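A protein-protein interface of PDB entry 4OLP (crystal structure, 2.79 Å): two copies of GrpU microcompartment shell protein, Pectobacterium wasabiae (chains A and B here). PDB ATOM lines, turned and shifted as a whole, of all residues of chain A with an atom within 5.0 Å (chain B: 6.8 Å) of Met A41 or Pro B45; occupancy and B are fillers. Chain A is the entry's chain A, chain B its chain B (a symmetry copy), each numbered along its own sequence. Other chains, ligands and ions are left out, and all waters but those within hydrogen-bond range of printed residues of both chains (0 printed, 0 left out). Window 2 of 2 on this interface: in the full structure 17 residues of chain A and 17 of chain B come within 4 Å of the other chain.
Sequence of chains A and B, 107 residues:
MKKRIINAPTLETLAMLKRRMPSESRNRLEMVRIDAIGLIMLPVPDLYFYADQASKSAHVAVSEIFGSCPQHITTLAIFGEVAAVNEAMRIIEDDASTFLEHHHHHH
Among the printed residues, pairs that only touch across the chains: Arg A4 with Phe B49 (3.1 Å), Thr A75 with Val B44 (3.3 Å), Met A41 with Pro B45 (3.4 Å), Lys A2 with Asp B46 (3.7 Å), Leu A39 with Pro B45 (3.8 Å), Leu A39 with Tyr B48 (3.8 Å) and Lys A2 with Pro B45 (3.8 Å).
Met A41 touches just one residue of chain B: Pro B45. Pro B45 touches just these residues of chain A: Lys A2, Leu A39 and Met A41. Printed residues of chain A within 4 Å of Asp B46: Lys A2 (3.7 Å) and Arg A4 (3.1 Å). Of the printed residues of chain B, Thr A75 touches Val B44 (3.3 Å). Leu B47 touches none of the printed residues of chain A. The nearest residue of chain B that does not touch Met A41 is Pro B43 (4.3 Å).
Of the 11 printed residues of chain A, 5 touch a printed residue of chain B. Printed residues of chain A that touch a printed residue of chain B: Lys A2, Arg A4, Leu A39, Met A41 and Thr A75. Hydrophobic or aromatic side chains of chain B that line the printed part of chain A: Val B44, Pro B45, Tyr B48, Phe B49 and Tyr B50. Along chain B the printed residues that touch a printed residue of chain A span positions 44 to 50.
The side-chain carboxylate of Asp B46 lies within salt-bridge range of the guanidinium group of Arg A4, at 3.1 Å. NH2 of Arg A4 is in hydrogen-bond range of OH of Tyr B50 (2.8 Å).
3 positions are printed for both chains. Of the 9 pairs that touch across the chains among the printed residues, none has its exchanged pair printed and touching as well.
The backbone carbonyl oxygen (O) of Lys A2 sits at hydrogen-bond distance from the backbone NH (N) of Met A41 (3.4 Å). The backbone NH of Leu A39 is in hydrogen-bond range of the backbone carbonyl oxygen of Arg A4, at 2.7 Å. OG1 of Thr A75 lies within hydrogen-bond range of SD of Met A41 (3.3 Å).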
ATOM      1  N   LYS A   2      12.432  -7.601  10.779  1.00  0.00           N
ATOM      2  CA  LYS A   2      13.827  -8.151  10.954  1.00  0.00           C
ATOM      3  C   LYS A   2      13.859  -9.432  11.815  1.00  0.00           C
ATOM      4  O   LYS A   2      12.903 -10.201  11.798  1.00  0.00           O
ATOM      5  CB  LYS A   2      14.760  -7.079  11.555  1.00  0.00           C
ATOM      6  CG  LYS A   2      14.390  -6.585  12.942  1.00  0.00           C
ATOM      7  CD  LYS A   2      15.505  -5.738  13.517  1.00  0.00           C
ATOM      8  CE  LYS A   2      15.227  -5.356  14.948  1.00  0.00           C
ATOM      9  NZ  LYS A   2      16.287  -4.446  15.454  1.00  0.00           N
ATOM     10  N   LYS A   3      14.964  -9.666  12.538  1.00  0.00           N
ATOM     11  CA  LYS A   3      15.118 -10.836  13.421  1.00  0.00           C
ATOM     12  C   LYS A   3      15.336 -10.469  14.893  1.00  0.00           C
ATOM     13  O   LYS A   3      15.839  -9.403  15.195  1.00  0.00           O
ATOM     14  CB  LYS A   3      16.247 -11.755  12.930  1.00  0.00           C
ATOM     15  CG  LYS A   3      17.643 -11.228  13.216  1.00  0.00           C
ATOM     16  CD  LYS A   3      18.729 -12.024  12.522  1.00  0.00           C
ATOM     17  CE  LYS A   3      20.080 -11.430  12.855  1.00  0.00           C
ATOM     18  NZ  LYS A   3      21.166 -12.061  12.062  1.00  0.00           N
ATOM     19  N   ARG A   4      14.967 -11.380  15.792  1.00  0.00           N
ATOM     20  CA  ARG A   4      15.006 -11.141  17.240  1.00  0.00           C
ATOM     21  C   ARG A   4      15.079 -12.452  17.986  1.00  0.00           C
ATOM     22  O   ARG A   4      14.462 -13.441  17.575  1.00  0.00           O
ATOM     23  CB  ARG A   4      13.716 -10.486  17.698  1.00  0.00           C
ATOM     24  CG  ARG A   4      13.647  -8.997  17.539  1.00  0.00           C
ATOM     25  CD  ARG A   4      14.383  -8.273  18.623  1.00  0.00           C
ATOM     26  NE  ARG A   4      14.116  -6.857  18.408  1.00  0.00           N
ATOM     27  CZ  ARG A   4      14.698  -5.864  19.058  1.00  0.00           C
ATOM     28  NH1 ARG A   4      15.622  -6.113  19.975  1.00  0.00           N
ATOM     29  NH2 ARG A   4      14.352  -4.612  18.787  1.00  0.00           N
ATOM     30  N   LEU A  39      12.860 -15.264  16.448  1.00  0.00           N
ATOM     31  CA  LEU A  39      11.753 -14.859  15.628  1.00  0.00           C
ATOM     32  C   LEU A  39      12.316 -14.146  14.437  1.00  0.00           C
ATOM     33  O   LEU A  39      13.086 -13.200  14.602  1.00  0.00           O
ATOM     34  CB  LEU A  39      10.856 -13.919  16.416  1.00  0.00           C
ATOM     35  CG  LEU A  39      10.251 -14.515  17.678  1.00  0.00           C
ATOM     36  CD1 LEU A  39       9.532 -13.446  18.486  1.00  0.00           C
ATOM     37  CD2 LEU A  39       9.305 -15.634  17.306  1.00  0.00           C
ATOM     38  N   ILE A  40      11.927 -14.578  13.244  1.00  0.00           N
ATOM     39  CA  ILE A  40      12.412 -13.949  12.028  1.00  0.00           C
ATOM     40  C   ILE A  40      11.324 -13.898  10.978  1.00  0.00           C
ATOM     41  O   ILE A  40      10.540 -14.837  10.835  1.00  0.00           O
ATOM     42  CB  ILE A  40      13.668 -14.664  11.507  1.00  0.00           C
ATOM     43  CG1 ILE A  40      14.149 -14.032  10.194  1.00  0.00           C
ATOM     44  CG2 ILE A  40      13.418 -16.152  11.331  1.00  0.00           C
ATOM     45  CD1 ILE A  40      15.644 -14.163   9.979  1.00  0.00           C
ATOM     46  N   MET A  41      11.262 -12.774  10.274  1.00  0.00           N
ATOM     47  CA  MET A  41      10.261 -12.560   9.258  1.00  0.00           C
ATOM     48  C   MET A  41      10.782 -12.978   7.902  1.00  0.00           C
ATOM     49  O   MET A  41      11.777 -12.444   7.432  1.00  0.00           O
ATOM     50  CB  MET A  41       9.937 -11.073   9.194  1.00  0.00           C
ATOM     51  CG  MET A  41       9.425 -10.474  10.524  1.00  0.00           C
ATOM     52  SD  MET A  41       7.645 -10.227  10.566  1.00  0.00           S
ATOM     53  CE  MET A  41       7.375  -8.712   9.640  1.00  0.00           C
ATOM     54  N   LEU A  42      10.061 -13.883   7.251  1.00  0.00           N
ATOM     55  CA  LEU A  42      10.502 -14.487   6.011  1.00  0.00           C
ATOM     56  C   LEU A  42       9.361 -14.567   5.011  1.00  0.00           C
ATOM     57  O   LEU A  42       8.201 -14.763   5.404  1.00  0.00           O
ATOM     58  CB  LEU A  42      10.976 -15.912   6.290  1.00  0.00           C
ATOM     59  CG  LEU A  42      12.285 -16.069   7.059  1.00  0.00           C
ATOM     60  CD1 LEU A  42      12.474 -17.502   7.534  1.00  0.00           C
ATOM     61  CD2 LEU A  42      13.467 -15.634   6.197  1.00  0.00           C
ATOM     62  N   PRO A  43       9.676 -14.453   3.708  1.00  0.00           N
ATOM     63  CA  PRO A  43       8.684 -14.834   2.688  1.00  0.00           C
ATOM     64  C   PRO A  43       8.362 -16.326   2.804  1.00  0.00           C
ATOM     65  O   PRO A  43       9.163 -17.088   3.357  1.00  0.00           O
ATOM     66  CB  PRO A  43       9.392 -14.527   1.359  1.00  0.00           C
ATOM     67  CG  PRO A  43      10.616 -13.748   1.701  1.00  0.00           C
ATOM     68  CD  PRO A  43      10.973 -14.086   3.112  1.00  0.00           C
ATOM     69  N   ILE A  73       4.708 -12.105   3.617  1.00  0.00           N
ATOM     70  CA  ILE A  73       5.906 -12.254   4.435  1.00  0.00           C
ATOM     71  C   ILE A  73       5.406 -12.553   5.847  1.00  0.00           C
ATOM     72  O   ILE A  73       4.725 -11.726   6.438  1.00  0.00           O
ATOM     73  CB  ILE A  73       6.736 -10.939   4.393  1.00  0.00           C
ATOM     74  CG1 ILE A  73       7.144 -10.608   2.945  1.00  0.00           C
ATOM     75  CG2 ILE A  73       7.971 -11.031   5.280  1.00  0.00           C
ATOM     76  CD1 ILE A  73       6.901  -9.163   2.534  1.00  0.00           C
ATOM     77  N   THR A  74       5.711 -13.734   6.382  1.00  0.00           N
ATOM     78  CA  THR A  74       5.178 -14.155   7.695  1.00  0.00           C
ATOM     79  C   THR A  74       6.347 -14.412   8.652  1.00  0.00           C
ATOM     80  O   THR A  74       7.480 -14.045   8.347  1.00  0.00           O
ATOM     81  CB  THR A  74       4.180 -15.366   7.581  1.00  0.00           C
ATOM     82  OG1 THR A  74       3.638 -15.699   8.869  1.00  0.00           O
ATOM     83  CG2 THR A  74       4.834 -16.603   6.988  1.00  0.00           C
ATOM     84  N   THR A  75       6.070 -14.993   9.817  1.00  0.00           N
ATOM     85  CA  THR A  75       7.088 -15.141  10.869  1.00  0.00           C
ATOM     86  C   THR A  75       7.361 -16.597  11.235  1.00  0.00           C
ATOM     87  O   THR A  75       6.440 -17.381  11.412  1.00  0.00           O
ATOM     88  CB  THR A  75       6.691 -14.371  12.144  1.00  0.00           C
ATOM     89  OG1 THR A  75       6.412 -13.013  11.807  1.00  0.00           O
ATOM     90  CG2 THR A  75       7.794 -14.392  13.182  1.00  0.00           C
ATOM     91  N   LEU B  42       4.278  -2.381  16.078  1.00  0.00           N
ATOM     92  CA  LEU B  42       5.542  -3.106  15.939  1.00  0.00           C
ATOM     93  C   LEU B  42       5.390  -4.291  15.015  1.00  0.00           C
ATOM     94  O   LEU B  42       4.306  -4.893  14.975  1.00  0.00           O
ATOM     95  CB  LEU B  42       5.988  -3.636  17.289  1.00  0.00           C
ATOM     96  CG  LEU B  42       6.502  -2.619  18.301  1.00  0.00           C
ATOM     97  CD1 LEU B  42       6.586  -3.237  19.696  1.00  0.00           C
ATOM     98  CD2 LEU B  42       7.857  -2.082  17.875  1.00  0.00           C
ATOM     99  N   PRO B  43       6.477  -4.638  14.275  1.00  0.00           N
ATOM    100  CA  PRO B  43       6.497  -5.929  13.579  1.00  0.00           C
ATOM    101  C   PRO B  43       6.462  -7.051  14.608  1.00  0.00           C
ATOM    102  O   PRO B  43       6.811  -6.830  15.779  1.00  0.00           O
ATOM    103  CB  PRO B  43       7.840  -5.924  12.821  1.00  0.00           C
ATOM    104  CG  PRO B  43       8.362  -4.532  12.890  1.00  0.00           C
ATOM    105  CD  PRO B  43       7.751  -3.907  14.106  1.00  0.00           C
ATOM    106  N   VAL B  44       6.053  -8.246  14.208  1.00  0.00           N
ATOM    107  CA  VAL B  44       5.735  -9.231  15.240  1.00  0.00           C
ATOM    108  C   VAL B  44       6.974  -9.719  16.005  1.00  0.00           C
ATOM    109  O   VAL B  44       6.870  -9.943  17.203  1.00  0.00           O
ATOM    110  CB  VAL B  44       4.785 -10.390  14.784  1.00  0.00           C
ATOM    111  CG1 VAL B  44       4.083 -10.062  13.469  1.00  0.00           C
ATOM    112  CG2 VAL B  44       5.491 -11.746  14.736  1.00  0.00           C
ATOM    113  N   PRO B  45       8.140  -9.852  15.352  1.00  0.00           N
ATOM    114  CA  PRO B  45       9.284 -10.273  16.179  1.00  0.00           C
ATOM    115  C   PRO B  45       9.588  -9.292  17.311  1.00  0.00           C
ATOM    116  O   PRO B  45       9.747  -9.702  18.463  1.00  0.00           O
ATOM    117  CB  PRO B  45      10.438 -10.328  15.173  1.00  0.00           C
ATOM    118  CG  PRO B  45       9.776 -10.684  13.900  1.00  0.00           C
ATOM    119  CD  PRO B  45       8.458  -9.934  13.915  1.00  0.00           C
ATOM    120  N   ASP B  46       9.592  -8.001  16.985  1.00  0.00           N
ATOM    121  CA  ASP B  46       9.778  -6.945  17.984  1.00  0.00           C
ATOM    122  C   ASP B  46       8.689  -7.000  19.052  1.00  0.00           C
ATOM    123  O   ASP B  46       8.972  -6.821  20.234  1.00  0.00           O
ATOM    124  CB  ASP B  46       9.749  -5.564  17.324  1.00  0.00           C
ATOM    125  CG  ASP B  46      11.064  -5.198  16.621  1.00  0.00           C
ATOM    126  OD1 ASP B  46      11.921  -6.081  16.391  1.00  0.00           O
ATOM    127  OD2 ASP B  46      11.214  -4.007  16.269  1.00  0.00           O
ATOM    128  N   LEU B  47       7.452  -7.264  18.622  1.00  0.00           N
ATOM    129  CA  LEU B  47       6.307  -7.260  19.516  1.00  0.00           C
ATOM    130  C   LEU B  47       6.524  -8.218  20.683  1.00  0.00           C
ATOM    131  O   LEU B  47       6.446  -7.836  21.854  1.00  0.00           O
ATOM    132  CB  LEU B  47       5.045  -7.652  18.779  1.00  0.00           C
ATOM    133  CG  LEU B  47       3.793  -7.549  19.659  1.00  0.00           C
ATOM    134  CD1 LEU B  47       2.992  -6.337  19.245  1.00  0.00           C
ATOM    135  CD2 LEU B  47       2.917  -8.792  19.578  1.00  0.00           C
ATOM    136  N   TYR B  48       6.827  -9.464  20.362  1.00  0.00           N
ATOM    137  CA  TYR B  48       7.027 -10.471  21.384  1.00  0.00           C
ATOM    138  C   TYR B  48       8.327 -10.271  22.131  1.00  0.00           C
ATOM    139  O   TYR B  48       8.407 -10.598  23.317  1.00  0.00           O
ATOM    140  CB  TYR B  48       6.992 -11.854  20.774  1.00  0.00           C
ATOM    141  CG  TYR B  48       5.640 -12.157  20.237  1.00  0.00           C
ATOM    142  CD1 TYR B  48       4.545 -12.174  21.077  1.00  0.00           C
ATOM    143  CD2 TYR B  48       5.440 -12.401  18.891  1.00  0.00           C
ATOM    144  CE1 TYR B  48       3.286 -12.450  20.602  1.00  0.00           C
ATOM    145  CE2 TYR B  48       4.180 -12.674  18.400  1.00  0.00           C
ATOM    146  CZ  TYR B  48       3.112 -12.701  19.266  1.00  0.00           C
ATOM    147  OH  TYR B  48       1.852 -12.980  18.818  1.00  0.00           O
ATOM    148  N   PHE B  49       9.338  -9.727  21.457  1.00  0.00           N
ATOM    149  CA  PHE B  49      10.593  -9.410  22.138  1.00  0.00           C
ATOM    150  C   PHE B  49      10.345  -8.382  23.231  1.00  0.00           C
ATOM    151  O   PHE B  49      10.685  -8.602  24.394  1.00  0.00           O
ATOM    152  CB  PHE B  49      11.667  -8.913  21.169  1.00  0.00           C
ATOM    153  CG  PHE B  49      12.954  -8.576  21.850  1.00  0.00           C
ATOM    154  CD1 PHE B  49      13.819  -9.582  22.274  1.00  0.00           C
ATOM    155  CD2 PHE B  49      13.283  -7.258  22.124  1.00  0.00           C
ATOM    156  CE1 PHE B  49      15.002  -9.270  22.940  1.00  0.00           C
ATOM    157  CE2 PHE B  49      14.465  -6.945  22.783  1.00  0.00           C
ATOM    158  CZ  PHE B  49      15.322  -7.950  23.190  1.00  0.00           C
ATOM    159  N   TYR B  50       9.705  -7.289  22.857  1.00  0.00           N
ATOM    160  CA  TYR B  50       9.455  -6.232  23.810  1.00  0.00           C
ATOM    161  C   TYR B  50       8.373  -6.578  24.833  1.00  0.00           C
ATOM    162  O   TYR B  50       8.459  -6.115  25.961  1.00  0.00           O
ATOM    163  CB  TYR B  50       9.186  -4.907  23.086  1.00  0.00           C
ATOM    164  CG  TYR B  50      10.452  -4.311  22.499  1.00  0.00           C
ATOM    165  CD1 TYR B  50      11.507  -3.932  23.321  1.00  0.00           C
ATOM    166  CD2 TYR B  50      10.594  -4.150  21.122  1.00  0.00           C
ATOM    167  CE1 TYR B  50      12.665  -3.403  22.774  1.00  0.00           C
ATOM    168  CE2 TYR B  50      11.744  -3.626  20.571  1.00  0.00           C
ATOM    169  CZ  TYR B  50      12.782  -3.252  21.397  1.00  0.00           C
ATOM    170  OH  TYR B  50      13.930  -2.714  20.834  1.00  0.00           O
ATOM    171  N   ILE B  73       2.538  -6.073  10.904  1.00  0.00           N
ATOM    172  CA  ILE B  73       2.805  -5.020  11.875  1.00  0.00           C
ATOM    173  C   ILE B  73       1.534  -4.817  12.725  1.00  0.00           C
ATOM    174  O   ILE B  73       0.514  -4.387  12.205  1.00  0.00           O
ATOM    175  CB  ILE B  73       3.201  -3.705  11.148  1.00  0.00           C
ATOM    176  CG1 ILE B  73       4.394  -3.936  10.197  1.00  0.00           C
ATOM    177  CG2 ILE B  73       3.532  -2.609  12.153  1.00  0.00           C
ATOM    178  CD1 ILE B  73       4.231  -3.332   8.813  1.00  0.00           C
